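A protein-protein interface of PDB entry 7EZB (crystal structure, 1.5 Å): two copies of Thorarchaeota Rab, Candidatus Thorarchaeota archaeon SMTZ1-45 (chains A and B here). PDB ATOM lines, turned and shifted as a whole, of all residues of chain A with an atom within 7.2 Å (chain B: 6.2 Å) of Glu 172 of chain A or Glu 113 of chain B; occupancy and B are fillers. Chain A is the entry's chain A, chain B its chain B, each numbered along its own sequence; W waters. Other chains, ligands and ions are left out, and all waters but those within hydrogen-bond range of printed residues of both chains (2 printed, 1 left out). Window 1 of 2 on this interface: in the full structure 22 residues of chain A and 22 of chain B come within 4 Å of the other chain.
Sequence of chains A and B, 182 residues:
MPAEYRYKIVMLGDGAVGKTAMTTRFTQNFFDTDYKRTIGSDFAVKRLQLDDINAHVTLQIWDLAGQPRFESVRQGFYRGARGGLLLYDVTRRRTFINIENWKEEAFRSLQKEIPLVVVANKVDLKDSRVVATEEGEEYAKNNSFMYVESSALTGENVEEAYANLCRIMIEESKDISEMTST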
ATOM      1  N   TYR A   7      14.915  24.238  20.952  1.00  0.00           N
ATOM      2  CA  TYR A   7      14.945  23.599  19.640  1.00  0.00           C
ATOM      3  C   TYR A   7      15.082  24.603  18.509  1.00  0.00           C
ATOM      4  O   TYR A   7      14.486  25.680  18.544  1.00  0.00           O
ATOM      5  CB  TYR A   7      13.661  22.810  19.345  1.00  0.00           C
ATOM      6  CG  TYR A   7      13.331  21.755  20.376  1.00  0.00           C
ATOM      7  CD1 TYR A   7      14.064  20.579  20.448  1.00  0.00           C
ATOM      8  CD2 TYR A   7      12.282  21.930  21.284  1.00  0.00           C
ATOM      9  CE1 TYR A   7      13.767  19.602  21.394  1.00  0.00           C
ATOM     10  CE2 TYR A   7      11.967  20.953  22.217  1.00  0.00           C
ATOM     11  CZ  TYR A   7      12.714  19.793  22.274  1.00  0.00           C
ATOM     12  OH  TYR A   7      12.418  18.827  23.213  1.00  0.00           O
ATOM     13  N   ARG A  82      15.449  20.164  14.730  1.00  0.00           N
ATOM     14  CA  ARG A  82      14.766  19.039  15.365  1.00  0.00           C
ATOM     15  C   ARG A  82      13.310  18.909  14.936  1.00  0.00           C
ATOM     16  O   ARG A  82      12.612  18.000  15.395  1.00  0.00           O
ATOM     17  CB  ARG A  82      14.903  19.116  16.895  1.00  0.00           C
ATOM     18  CG  ARG A  82      16.288  18.690  17.428  1.00  0.00           C
ATOM     19  CD  ARG A  82      16.360  17.179  17.593  1.00  0.00           C
ATOM     20  NE  ARG A  82      15.194  16.691  18.328  1.00  0.00           N
ATOM     21  CZ  ARG A  82      15.175  16.433  19.633  1.00  0.00           C
ATOM     22  NH1 ARG A  82      16.274  16.586  20.362  1.00  0.00           N
ATOM     23  NH2 ARG A  82      14.047  16.017  20.208  1.00  0.00           N
ATOM     24  N   GLU A 113      15.201  11.492   9.490  1.00  0.00           N
ATOM     25  CA  GLU A 113      13.873  12.078   9.553  1.00  0.00           C
ATOM     26  C   GLU A 113      13.784  12.989  10.774  1.00  0.00           C
ATOM     27  O   GLU A 113      14.400  12.728  11.811  1.00  0.00           O
ATOM     28  CB  GLU A 113      12.829  10.968   9.660  1.00  0.00           C
ATOM     29  CG  GLU A 113      12.747  10.102   8.415  1.00  0.00           C
ATOM     30  CD  GLU A 113      12.008   8.804   8.652  1.00  0.00           C
ATOM     31  OE1 GLU A 113      12.663   7.741   8.622  1.00  0.00           O
ATOM     32  OE2 GLU A 113      10.779   8.846   8.877  1.00  0.00           O
ATOM     33  N   ILE A 114      13.051  14.082  10.629  1.00  0.00           N
ATOM     34  CA  ILE A 114      12.672  14.915  11.774  1.00  0.00           C
ATOM     35  C   ILE A 114      11.161  15.072  11.719  1.00  0.00           C
ATOM     36  O   ILE A 114      10.575  14.982  10.634  1.00  0.00           O
ATOM     37  CB  ILE A 114      13.355  16.293  11.766  1.00  0.00           C
ATOM     38  CG1 ILE A 114      13.059  17.036  10.455  1.00  0.00           C
ATOM     39  CG2 ILE A 114      14.846  16.146  12.048  1.00  0.00           C
ATOM     40  CD1 ILE A 114      13.480  18.523  10.462  1.00  0.00           C
ATOM     41  N   PRO A 115      10.494  15.324  12.842  1.00  0.00           N
ATOM     42  CA  PRO A 115       9.043  15.519  12.782  1.00  0.00           C
ATOM     43  C   PRO A 115       8.680  16.768  12.005  1.00  0.00           C
ATOM     44  O   PRO A 115       9.306  17.818  12.152  1.00  0.00           O
ATOM     45  CB  PRO A 115       8.633  15.650  14.254  1.00  0.00           C
ATOM     46  CG  PRO A 115       9.899  16.035  14.982  1.00  0.00           C
ATOM     47  CD  PRO A 115      11.027  15.377  14.217  1.00  0.00           C
ATOM     48  N   CYS A 166       6.127  21.475  18.988  1.00  0.00           N
ATOM     49  CA  CYS A 166       6.884  21.508  20.236  1.00  0.00           C
ATOM     50  C   CYS A 166       6.617  20.262  21.063  1.00  0.00           C
ATOM     51  O   CYS A 166       7.552  19.665  21.611  1.00  0.00           O
ATOM     52  CB  CYS A 166       6.496  22.728  21.057  1.00  0.00           C
ATOM     53  SG  CYS A 166       7.237  24.256  20.421  1.00  0.00           S
ATOM     54  N   ARG A 167       5.346  19.876  21.204  1.00  0.00           N
ATOM     55  CA  ARG A 167       5.050  18.705  22.025  1.00  0.00           C
ATOM     56  C   ARG A 167       5.686  17.455  21.431  1.00  0.00           C
ATOM     57  O   ARG A 167       6.225  16.614  22.167  1.00  0.00           O
ATOM     58  CB  ARG A 167       3.544  18.517  22.188  1.00  0.00           C
ATOM     59  CG  ARG A 167       3.189  17.368  23.126  1.00  0.00           C
ATOM     60  CD  ARG A 167       3.872  17.535  24.483  1.00  0.00           C
ATOM     61  NE  ARG A 167       3.627  16.410  25.385  1.00  0.00           N
ATOM     62  CZ  ARG A 167       2.541  16.283  26.143  1.00  0.00           C
ATOM     63  NH1 ARG A 167       1.591  17.210  26.094  1.00  0.00           N
ATOM     64  NH2 ARG A 167       2.404  15.227  26.953  1.00  0.00           N
ATOM     65  N   ILE A 168       5.649  17.320  20.103  1.00  0.00           N
ATOM     66  CA  ILE A 168       6.269  16.168  19.460  1.00  0.00           C
ATOM     67  C   ILE A 168       7.762  16.139  19.735  1.00  0.00           C
ATOM     68  O   ILE A 168       8.333  15.079  20.033  1.00  0.00           O
ATOM     69  CB  ILE A 168       5.959  16.167  17.952  1.00  0.00           C
ATOM     70  CG1 ILE A 168       4.452  15.972  17.754  1.00  0.00           C
ATOM     71  CG2 ILE A 168       6.777  15.089  17.225  1.00  0.00           C
ATOM     72  CD1 ILE A 168       3.972  16.391  16.356  1.00  0.00           C
ATOM     73  N   MET A 169       8.419  17.297  19.625  1.00  0.00           N
ATOM     74  CA  MET A 169       9.866  17.337  19.838  1.00  0.00           C
ATOM     75  C   MET A 169      10.217  17.023  21.288  1.00  0.00           C
ATOM     76  O   MET A 169      11.212  16.338  21.553  1.00  0.00           O
ATOM     77  CB  MET A 169      10.441  18.696  19.417  1.00  0.00           C
ATOM     78  CG  MET A 169      10.338  18.933  17.917  1.00  0.00           C
ATOM     79  SD  MET A 169      11.134  20.453  17.369  1.00  0.00           S
ATOM     80  CE  MET A 169      10.182  21.665  18.291  1.00  0.00           C
ATOM     81  N   ILE A 170       9.397  17.482  22.235  1.00  0.00           N
ATOM     82  CA  ILE A 170       9.604  17.143  23.645  1.00  0.00           C
ATOM     83  C   ILE A 170       9.451  15.643  23.869  1.00  0.00           C
ATOM     84  O   ILE A 170      10.240  15.019  24.588  1.00  0.00           O
ATOM     85  CB  ILE A 170       8.627  17.947  24.525  1.00  0.00           C
ATOM     86  CG1 ILE A 170       9.041  19.414  24.584  1.00  0.00           C
ATOM     87  CG2 ILE A 170       8.540  17.340  25.930  1.00  0.00           C
ATOM     88  CD1 ILE A 170       7.968  20.298  25.231  1.00  0.00           C
ATOM     89  N   GLU A 171       8.401  15.044  23.297  1.00  0.00           N
ATOM     90  CA  GLU A 171       8.247  13.597  23.465  1.00  0.00           C
ATOM     91  C   GLU A 171       9.423  12.838  22.858  1.00  0.00           C
ATOM     92  O   GLU A 171       9.823  11.792  23.394  1.00  0.00           O
ATOM     93  CB  GLU A 171       6.912  13.120  22.892  1.00  0.00           C
ATOM     94  CG  GLU A 171       5.698  13.646  23.663  1.00  0.00           C
ATOM     95  CD  GLU A 171       5.789  13.377  25.186  1.00  0.00           C
ATOM     96  OE1 GLU A 171       6.046  12.214  25.586  1.00  0.00           O
ATOM     97  OE2 GLU A 171       5.600  14.327  25.988  1.00  0.00           O
ATOM     98  N   GLU A 172       9.989  13.342  21.749  1.00  0.00           N
ATOM     99  CA  GLU A 172      11.174  12.698  21.186  1.00  0.00           C
ATOM    100  C   GLU A 172      12.393  12.876  22.090  1.00  0.00           C
ATOM    101  O   GLU A 172      13.166  11.929  22.273  1.00  0.00           O
ATOM    102  CB  GLU A 172      11.395  13.129  19.731  1.00  0.00           C
ATOM    103  CG  GLU A 172      10.111  12.905  18.937  1.00  0.00           C
ATOM    104  CD  GLU A 172      10.261  12.785  17.437  1.00  0.00           C
ATOM    105  OE1 GLU A 172      11.263  13.265  16.866  1.00  0.00           O
ATOM    106  OE2 GLU A 172       9.335  12.201  16.832  1.00  0.00           O
ATOM    107  N   SER A 173      12.569  14.064  22.678  1.00  0.00           N
ATOM    108  CA  SER A 173      13.633  14.269  23.659  1.00  0.00           C
ATOM    109  C   SER A 173      13.506  13.283  24.809  1.00  0.00           C
ATOM    110  O   SER A 173      14.500  12.690  25.251  1.00  0.00           O
ATOM    111  CB  SER A 173      13.581  15.699  24.203  1.00  0.00           C
ATOM    112  OG  SER A 173      13.993  16.635  23.219  1.00  0.00           O
ATOM    113  N   LYS A 174      12.284  13.110  25.323  1.00  0.00           N
ATOM    114  CA  LYS A 174      12.069  12.130  26.385  1.00  0.00           C
ATOM    115  C   LYS A 174      12.404  10.716  25.920  1.00  0.00           C
ATOM    116  O   LYS A 174      13.009   9.941  26.676  1.00  0.00           O
ATOM    117  CB  LYS A 174      10.624  12.208  26.881  1.00  0.00           C
ATOM    118  CG  LYS A 174      10.312  13.495  27.603  1.00  0.00           C
ATOM    119  CD  LYS A 174       8.811  13.568  27.944  1.00  0.00           C
ATOM    120  CE  LYS A 174       8.486  14.800  28.741  1.00  0.00           C
ATOM    121  NZ  LYS A 174       7.003  14.862  29.015  1.00  0.00           N
ATOM    122  N   ASP A 175      11.984  10.350  24.701  1.00  0.00           N
ATOM    123  CA  ASP A 175      12.318   9.032  24.158  1.00  0.00           C
ATOM    124  C   ASP A 175      13.826   8.824  24.166  1.00  0.00           C
ATOM    125  O   ASP A 175      14.323   7.746  24.519  1.00  0.00           O
ATOM    126  CB  ASP A 175      11.849   8.886  22.705  1.00  0.00           C
ATOM    127  CG  ASP A 175      10.341   8.943  22.519  1.00  0.00           C
ATOM    128  OD1 ASP A 175       9.576   8.604  23.440  1.00  0.00           O
ATOM    129  OD2 ASP A 175       9.942   9.292  21.377  1.00  0.00           O
ATOM    130  N   ILE A 176      14.568   9.841  23.721  1.00  0.00           N
ATOM    131  CA  ILE A 176      16.021   9.728  23.661  1.00  0.00           C
ATOM    132  C   ILE A 176      16.610   9.594  25.065  1.00  0.00           C
ATOM    133  O   ILE A 176      17.523   8.787  25.299  1.00  0.00           O
ATOM    134  CB  ILE A 176      16.603  10.924  22.886  1.00  0.00           C
ATOM    135  CG1 ILE A 176      16.140  10.864  21.424  1.00  0.00           C
ATOM    136  CG2 ILE A 176      18.115  10.919  23.004  1.00  0.00           C
ATOM    137  CD1 ILE A 176      16.330  12.174  20.696  1.00  0.00           C
ATOM    138  N   SER A 177      16.076  10.339  26.028  1.00  0.00           N
ATOM    139  CA  SER A 177      16.543  10.190  27.407  1.00  0.00           C
ATOM    140  C   SER A 177      16.404   8.753  27.881  1.00  0.00           C
ATOM    141  O   SER A 177      17.291   8.213  28.561  1.00  0.00           O
ATOM    142  CB  SER A 177      15.731  11.099  28.326  1.00  0.00           C
ATOM    143  OG  SER A 177      16.026  12.468  28.098  1.00  0.00           O
ATOM    144  N   GLU A 178      15.287   8.114  27.540  1.00  0.00           N
ATOM    145  CA  GLU A 178      15.084   6.733  27.955  1.00  0.00           C
ATOM    146  C   GLU A 178      16.043   5.785  27.249  1.00  0.00           C
ATOM    147  O   GLU A 178      16.513   4.812  27.853  1.00  0.00           O
ATOM    148  CB  GLU A 178      13.632   6.347  27.702  1.00  0.00           C
ATOM    149  CG  GLU A 178      12.714   7.123  28.635  1.00  0.00           C
ATOM    150  CD  GLU A 178      11.429   7.571  27.981  1.00  0.00           C
ATOM    151  OE1 GLU A 178      11.156   7.152  26.841  1.00  0.00           O
ATOM    152  OE2 GLU A 178      10.686   8.348  28.616  1.00  0.00           O
ATOM    153  N   MET A 179      16.344   6.050  25.982  1.00  0.00           N
ATOM    154  CA  MET A 179      17.242   5.172  25.242  1.00  0.00           C
ATOM    155  C   MET A 179      18.662   5.251  25.775  1.00  0.00           C
ATOM    156  O   MET A 179      19.403   4.267  25.719  1.00  0.00           O
ATOM    157  CB  MET A 179      17.258   5.567  23.772  1.00  0.00           C
ATOM    158  CG  MET A 179      15.991   5.280  23.055  1.00  0.00           C
ATOM    159  SD  MET A 179      16.205   5.916  21.381  1.00  0.00           S
ATOM    160  CE  MET A 179      14.516   5.737  20.853  1.00  0.00           C
ATOM    161  N   PHE B 107      11.086   1.401  22.020  1.00  0.00           N
ATOM    162  CA  PHE B 107      12.119   2.347  21.606  1.00  0.00           C
ATOM    163  C   PHE B 107      13.439   2.092  22.336  1.00  0.00           C
ATOM    164  O   PHE B 107      14.520   2.207  21.733  1.00  0.00           O
ATOM    165  CB  PHE B 107      11.649   3.791  21.810  1.00  0.00           C
ATOM    166  CG  PHE B 107      10.498   4.214  20.913  1.00  0.00           C
ATOM    167  CD1 PHE B 107       9.934   3.349  19.987  1.00  0.00           C
ATOM    168  CD2 PHE B 107      10.014   5.513  20.990  1.00  0.00           C
ATOM    169  CE1 PHE B 107       8.880   3.784  19.172  1.00  0.00           C
ATOM    170  CE2 PHE B 107       8.984   5.953  20.185  1.00  0.00           C
ATOM    171  CZ  PHE B 107       8.408   5.099  19.285  1.00  0.00           C
ATOM    172  N   LEU B 110      15.032  -1.035  20.677  1.00  0.00           N
ATOM    173  CA  LEU B 110      15.528  -0.833  19.322  1.00  0.00           C
ATOM    174  C   LEU B 110      16.561   0.272  19.228  1.00  0.00           C
ATOM    175  O   LEU B 110      17.268   0.344  18.219  1.00  0.00           O
ATOM    176  CB  LEU B 110      14.366  -0.476  18.397  1.00  0.00           C
ATOM    177  CG  LEU B 110      13.370  -1.608  18.167  1.00  0.00           C
ATOM    178  CD1 LEU B 110      12.053  -1.056  17.592  1.00  0.00           C
ATOM    179  CD2 LEU B 110      14.005  -2.590  17.221  1.00  0.00           C
ATOM    180  N   GLN B 111      16.661   1.127  20.251  1.00  0.00           N
ATOM    181  CA  GLN B 111      17.505   2.319  20.240  1.00  0.00           C
ATOM    182  C   GLN B 111      17.134   3.277  19.117  1.00  0.00           C
ATOM    183  O   GLN B 111      17.977   4.033  18.636  1.00  0.00           O
ATOM    184  CB  GLN B 111      18.999   1.986  20.224  1.00  0.00           C
ATOM    185  CG  GLN B 111      19.456   1.301  21.482  1.00  0.00           C
ATOM    186  CD  GLN B 111      19.613   2.265  22.621  1.00  0.00           C
ATOM    187  OE1 GLN B 111      20.474   3.143  22.597  1.00  0.00           O
ATOM    188  NE2 GLN B 111      18.772   2.114  23.648  1.00  0.00           N
ATOM    189  N   LYS B 112      15.865   3.250  18.720  1.00  0.00           N
ATOM    190  CA  LYS B 112      15.354   4.202  17.756  1.00  0.00           C
ATOM    191  C   LYS B 112      13.838   4.227  17.895  1.00  0.00           C
ATOM    192  O   LYS B 112      13.234   3.315  18.460  1.00  0.00           O
ATOM    193  CB  LYS B 112      15.753   3.799  16.334  1.00  0.00           C
ATOM    194  CG  LYS B 112      15.138   2.466  15.930  1.00  0.00           C
ATOM    195  CD  LYS B 112      15.602   2.053  14.522  1.00  0.00           C
ATOM    196  CE  LYS B 112      14.984   0.716  14.134  1.00  0.00           C
ATOM    197  NZ  LYS B 112      15.274   0.395  12.695  1.00  0.00           N
ATOM    198  N   GLU B 113      13.242   5.285  17.355  1.00  0.00           N
ATOM    199  CA  GLU B 113      11.796   5.354  17.214  1.00  0.00           C
ATOM    200  C   GLU B 113      11.401   4.596  15.956  1.00  0.00           C
ATOM    201  O   GLU B 113      12.125   4.619  14.951  1.00  0.00           O
ATOM    202  CB  GLU B 113      11.378   6.811  17.056  1.00  0.00           C
ATOM    203  CG  GLU B 113      11.757   7.685  18.223  1.00  0.00           C
ATOM    204  CD  GLU B 113      11.594   9.149  17.879  1.00  0.00           C
ATOM    205  OE1 GLU B 113      10.438   9.613  17.776  1.00  0.00           O
ATOM    206  OE2 GLU B 113      12.623   9.822  17.673  1.00  0.00           O
ATOM    207  N   ILE B 114      10.286   3.879  16.035  1.00  0.00           N
ATOM    208  CA  ILE B 114       9.634   3.299  14.861  1.00  0.00           C
ATOM    209  C   ILE B 114       8.212   3.848  14.824  1.00  0.00           C
ATOM    210  O   ILE B 114       7.677   4.240  15.869  1.00  0.00           O
ATOM    211  CB  ILE B 114       9.603   1.762  14.904  1.00  0.00           C
ATOM    212  CG1 ILE B 114       9.000   1.271  16.212  1.00  0.00           C
ATOM    213  CG2 ILE B 114      11.005   1.197  14.680  1.00  0.00           C
ATOM    214  CD1 ILE B 114       8.700  -0.249  16.214  1.00  0.00           C
ATOM    215  N   PRO B 115       7.576   3.915  13.660  1.00  0.00           N
ATOM    216  CA  PRO B 115       6.195   4.408  13.617  1.00  0.00           C
ATOM    217  C   PRO B 115       5.267   3.446  14.328  1.00  0.00           C
ATOM    218  O   PRO B 115       5.353   2.222  14.163  1.00  0.00           O
ATOM    219  CB  PRO B 115       5.882   4.463  12.118  1.00  0.00           C
ATOM    220  CG  PRO B 115       6.850   3.487  11.495  1.00  0.00           C
ATOM    221  CD  PRO B 115       8.107   3.613  12.322  1.00  0.00           C
ATOM    222  N   ASN B 142       0.442  13.963  20.433  1.00  0.00           N
ATOM    223  CA  ASN B 142       1.645  14.375  21.160  1.00  0.00           C
ATOM    224  C   ASN B 142       2.884  13.621  20.697  1.00  0.00           C
ATOM    225  O   ASN B 142       4.006  14.100  20.927  1.00  0.00           O
ATOM    226  CB  ASN B 142       1.460  14.107  22.661  1.00  0.00           C
ATOM    227  CG  ASN B 142       0.392  14.984  23.309  1.00  0.00           C
ATOM    228  OD1 ASN B 142       0.005  16.037  22.792  1.00  0.00           O
ATOM    229  ND2 ASN B 142      -0.058  14.561  24.484  1.00  0.00           N
ATOM    230  N   ASN B 143       2.718  12.446  20.085  1.00  0.00           N
ATOM    231  CA  ASN B 143       3.835  11.631  19.611  1.00  0.00           C
ATOM    232  C   ASN B 143       3.916  11.590  18.089  1.00  0.00           C
ATOM    233  O   ASN B 143       4.720  10.823  17.539  1.00  0.00           O
ATOM    234  CB  ASN B 143       3.685  10.197  20.137  1.00  0.00           C
ATOM    235  CG  ASN B 143       3.990  10.090  21.607  1.00  0.00           C
ATOM    236  OD1 ASN B 143       5.153   9.950  21.995  1.00  0.00           O
ATOM    237  ND2 ASN B 143       2.958  10.182  22.450  1.00  0.00           N
ATOM    238  N   SER B 144       3.068  12.357  17.400  1.00  0.00           N
ATOM    239  CA  SER B 144       2.945  12.288  15.943  1.00  0.00           C
ATOM    240  C   SER B 144       2.589  10.882  15.458  1.00  0.00           C
ATOM    241  O   SER B 144       3.044  10.443  14.403  1.00  0.00           O
ATOM    242  CB  SER B 144       4.179  12.835  15.229  1.00  0.00           C
ATOM    243  OG  SER B 144       3.881  13.134  13.872  1.00  0.00           O
ATOM    244  N   GLU B 172       8.608   5.727   4.888  1.00  0.00           N
ATOM    245  CA  GLU B 172       9.896   5.759   5.576  1.00  0.00           C
ATOM    246  C   GLU B 172      10.967   5.015   4.783  1.00  0.00           C
ATOM    247  O   GLU B 172      12.114   5.472   4.697  1.00  0.00           O
ATOM    248  CB  GLU B 172       9.753   5.186   6.989  1.00  0.00           C
ATOM    249  CG  GLU B 172      11.029   5.220   7.811  1.00  0.00           C
ATOM    250  CD  GLU B 172      10.775   5.009   9.293  1.00  0.00           C
ATOM    251  OE1 GLU B 172       9.652   4.596   9.649  1.00  0.00           O
ATOM    252  OE2 GLU B 172      11.694   5.264  10.102  1.00  0.00           O
HETATM  253  O   HOH W   1       7.486   9.953  20.587  1.00  0.00           O
HETATM  254  O   HOH W   2       3.852  10.494  25.273  1.00  0.00           O
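Water W1 lies within hydrogen-bond range of the side-chain carboxylate of Asp 175 of chain A (2.7 Å) and the side-chain amide oxygen of Asn 143 of chain B (2.7 Å). Water W2 bridges the side-chain carboxylate (OE1) of Glu 171 of chain A (2.8 Å) and the side-chain amide nitrogen (ND2) of Asn 143 of chain B (3.0 Å).
Of the 11 printed residues of chain B, 8 touch a printed residue of chain A. Hydrophobic or aromatic side chains of chain B that line the printed part of chain A: Phe 107. Among the printed residues, 13 pairs touch across the chains.
Printed residues of chain B within 4 Å of Glu 172 of chain A: Glu 113. Printed residues of chain A within 4 Å of Glu 113 of chain B: Glu 172 (3.0 Å), Asp 175 (3.6 Å) and Met 179 (3.8 Å). Printed residues of chain B within 4 Å of Ile 168 of chain A: Asn 142 and Ser 144. Of the printed residues of chain B, Met 179 of chain A touches Phe 107, Gln 111, Lys 112 and Glu 113. Printed residues of chain B within 4 Å of Arg 167 of chain A: Asn 142 (3.5 Å). Printed residues of chain A within 4 Å of Phe 107 of chain B: Asp 175 and Met 179. Of the printed residues of chain A, Gln 111 of chain B touches Met 179.
Glu 113 of chain A touches Glu 172 of chain B, and with the chains exchanged Glu 172 of chain A touches Glu 113 of chain B. Positions printed for both chains: 113, 114, 115 and 172.
NE2 of Gln 111 of chain B is in hydrogen-bond range of O of Met 179 of chain A (3.1 Å). The side-chain sulfur of Met 179 of chain A sits close to the backbone NH of Lys 112 of chain B, 3.8 Å away. The side-chain carboxylate of Glu 172 of chain B sits close to the side-chain carboxylate of Glu 113 of chain A. The side-chain carboxylate (OE2) of Glu 172 of chain A sits close to the side-chain carboxylate (OE1) of Glu 113 of chain B.
OE2 of Glu 171 of chain A lies within salt-bridge range of NE of Arg 167 of chain A, at 2.9 Å. OE2 of Glu 171 of chain A is in salt-bridge range of NZ of Lys 174 of chain A, 3.4 Å away. The backbone carbonyl oxygen of Phe 107 of chain B lies within hydrogen-bond range of the backbone NH of Lys 112 of chain B, at 3.5 Å.
Asn 142 of chain B touches Arg 167 of chain A (OD1 to CG, 3.5 Å). CA of Ile 168 of chain A touches O of Asn 142 of chain B, 3.4 Å away. CB of Ser 144 of chain B touches CD1 of Ile 168 of chain A, 3.7 Å away. Asn 142 of chain B touches Glu 171 of chain A (O to CG, 3.2 Å). Asn 143 of chain B touches Glu 171 of chain A (OD1 to CB, 3.7 Å). Asp 175 of chain A touches Phe 107 of chain B. Glu 113 of chain B touches Asp 175 of chain A (OE1 to OD2, 3.6 Å). Phe 107 of chain B touches Met 179 of chain A (CB to CE, 3.6 Å). CE of Met 179 of chain A touches N of Glu 113 of chain B, at 3.8 Å.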
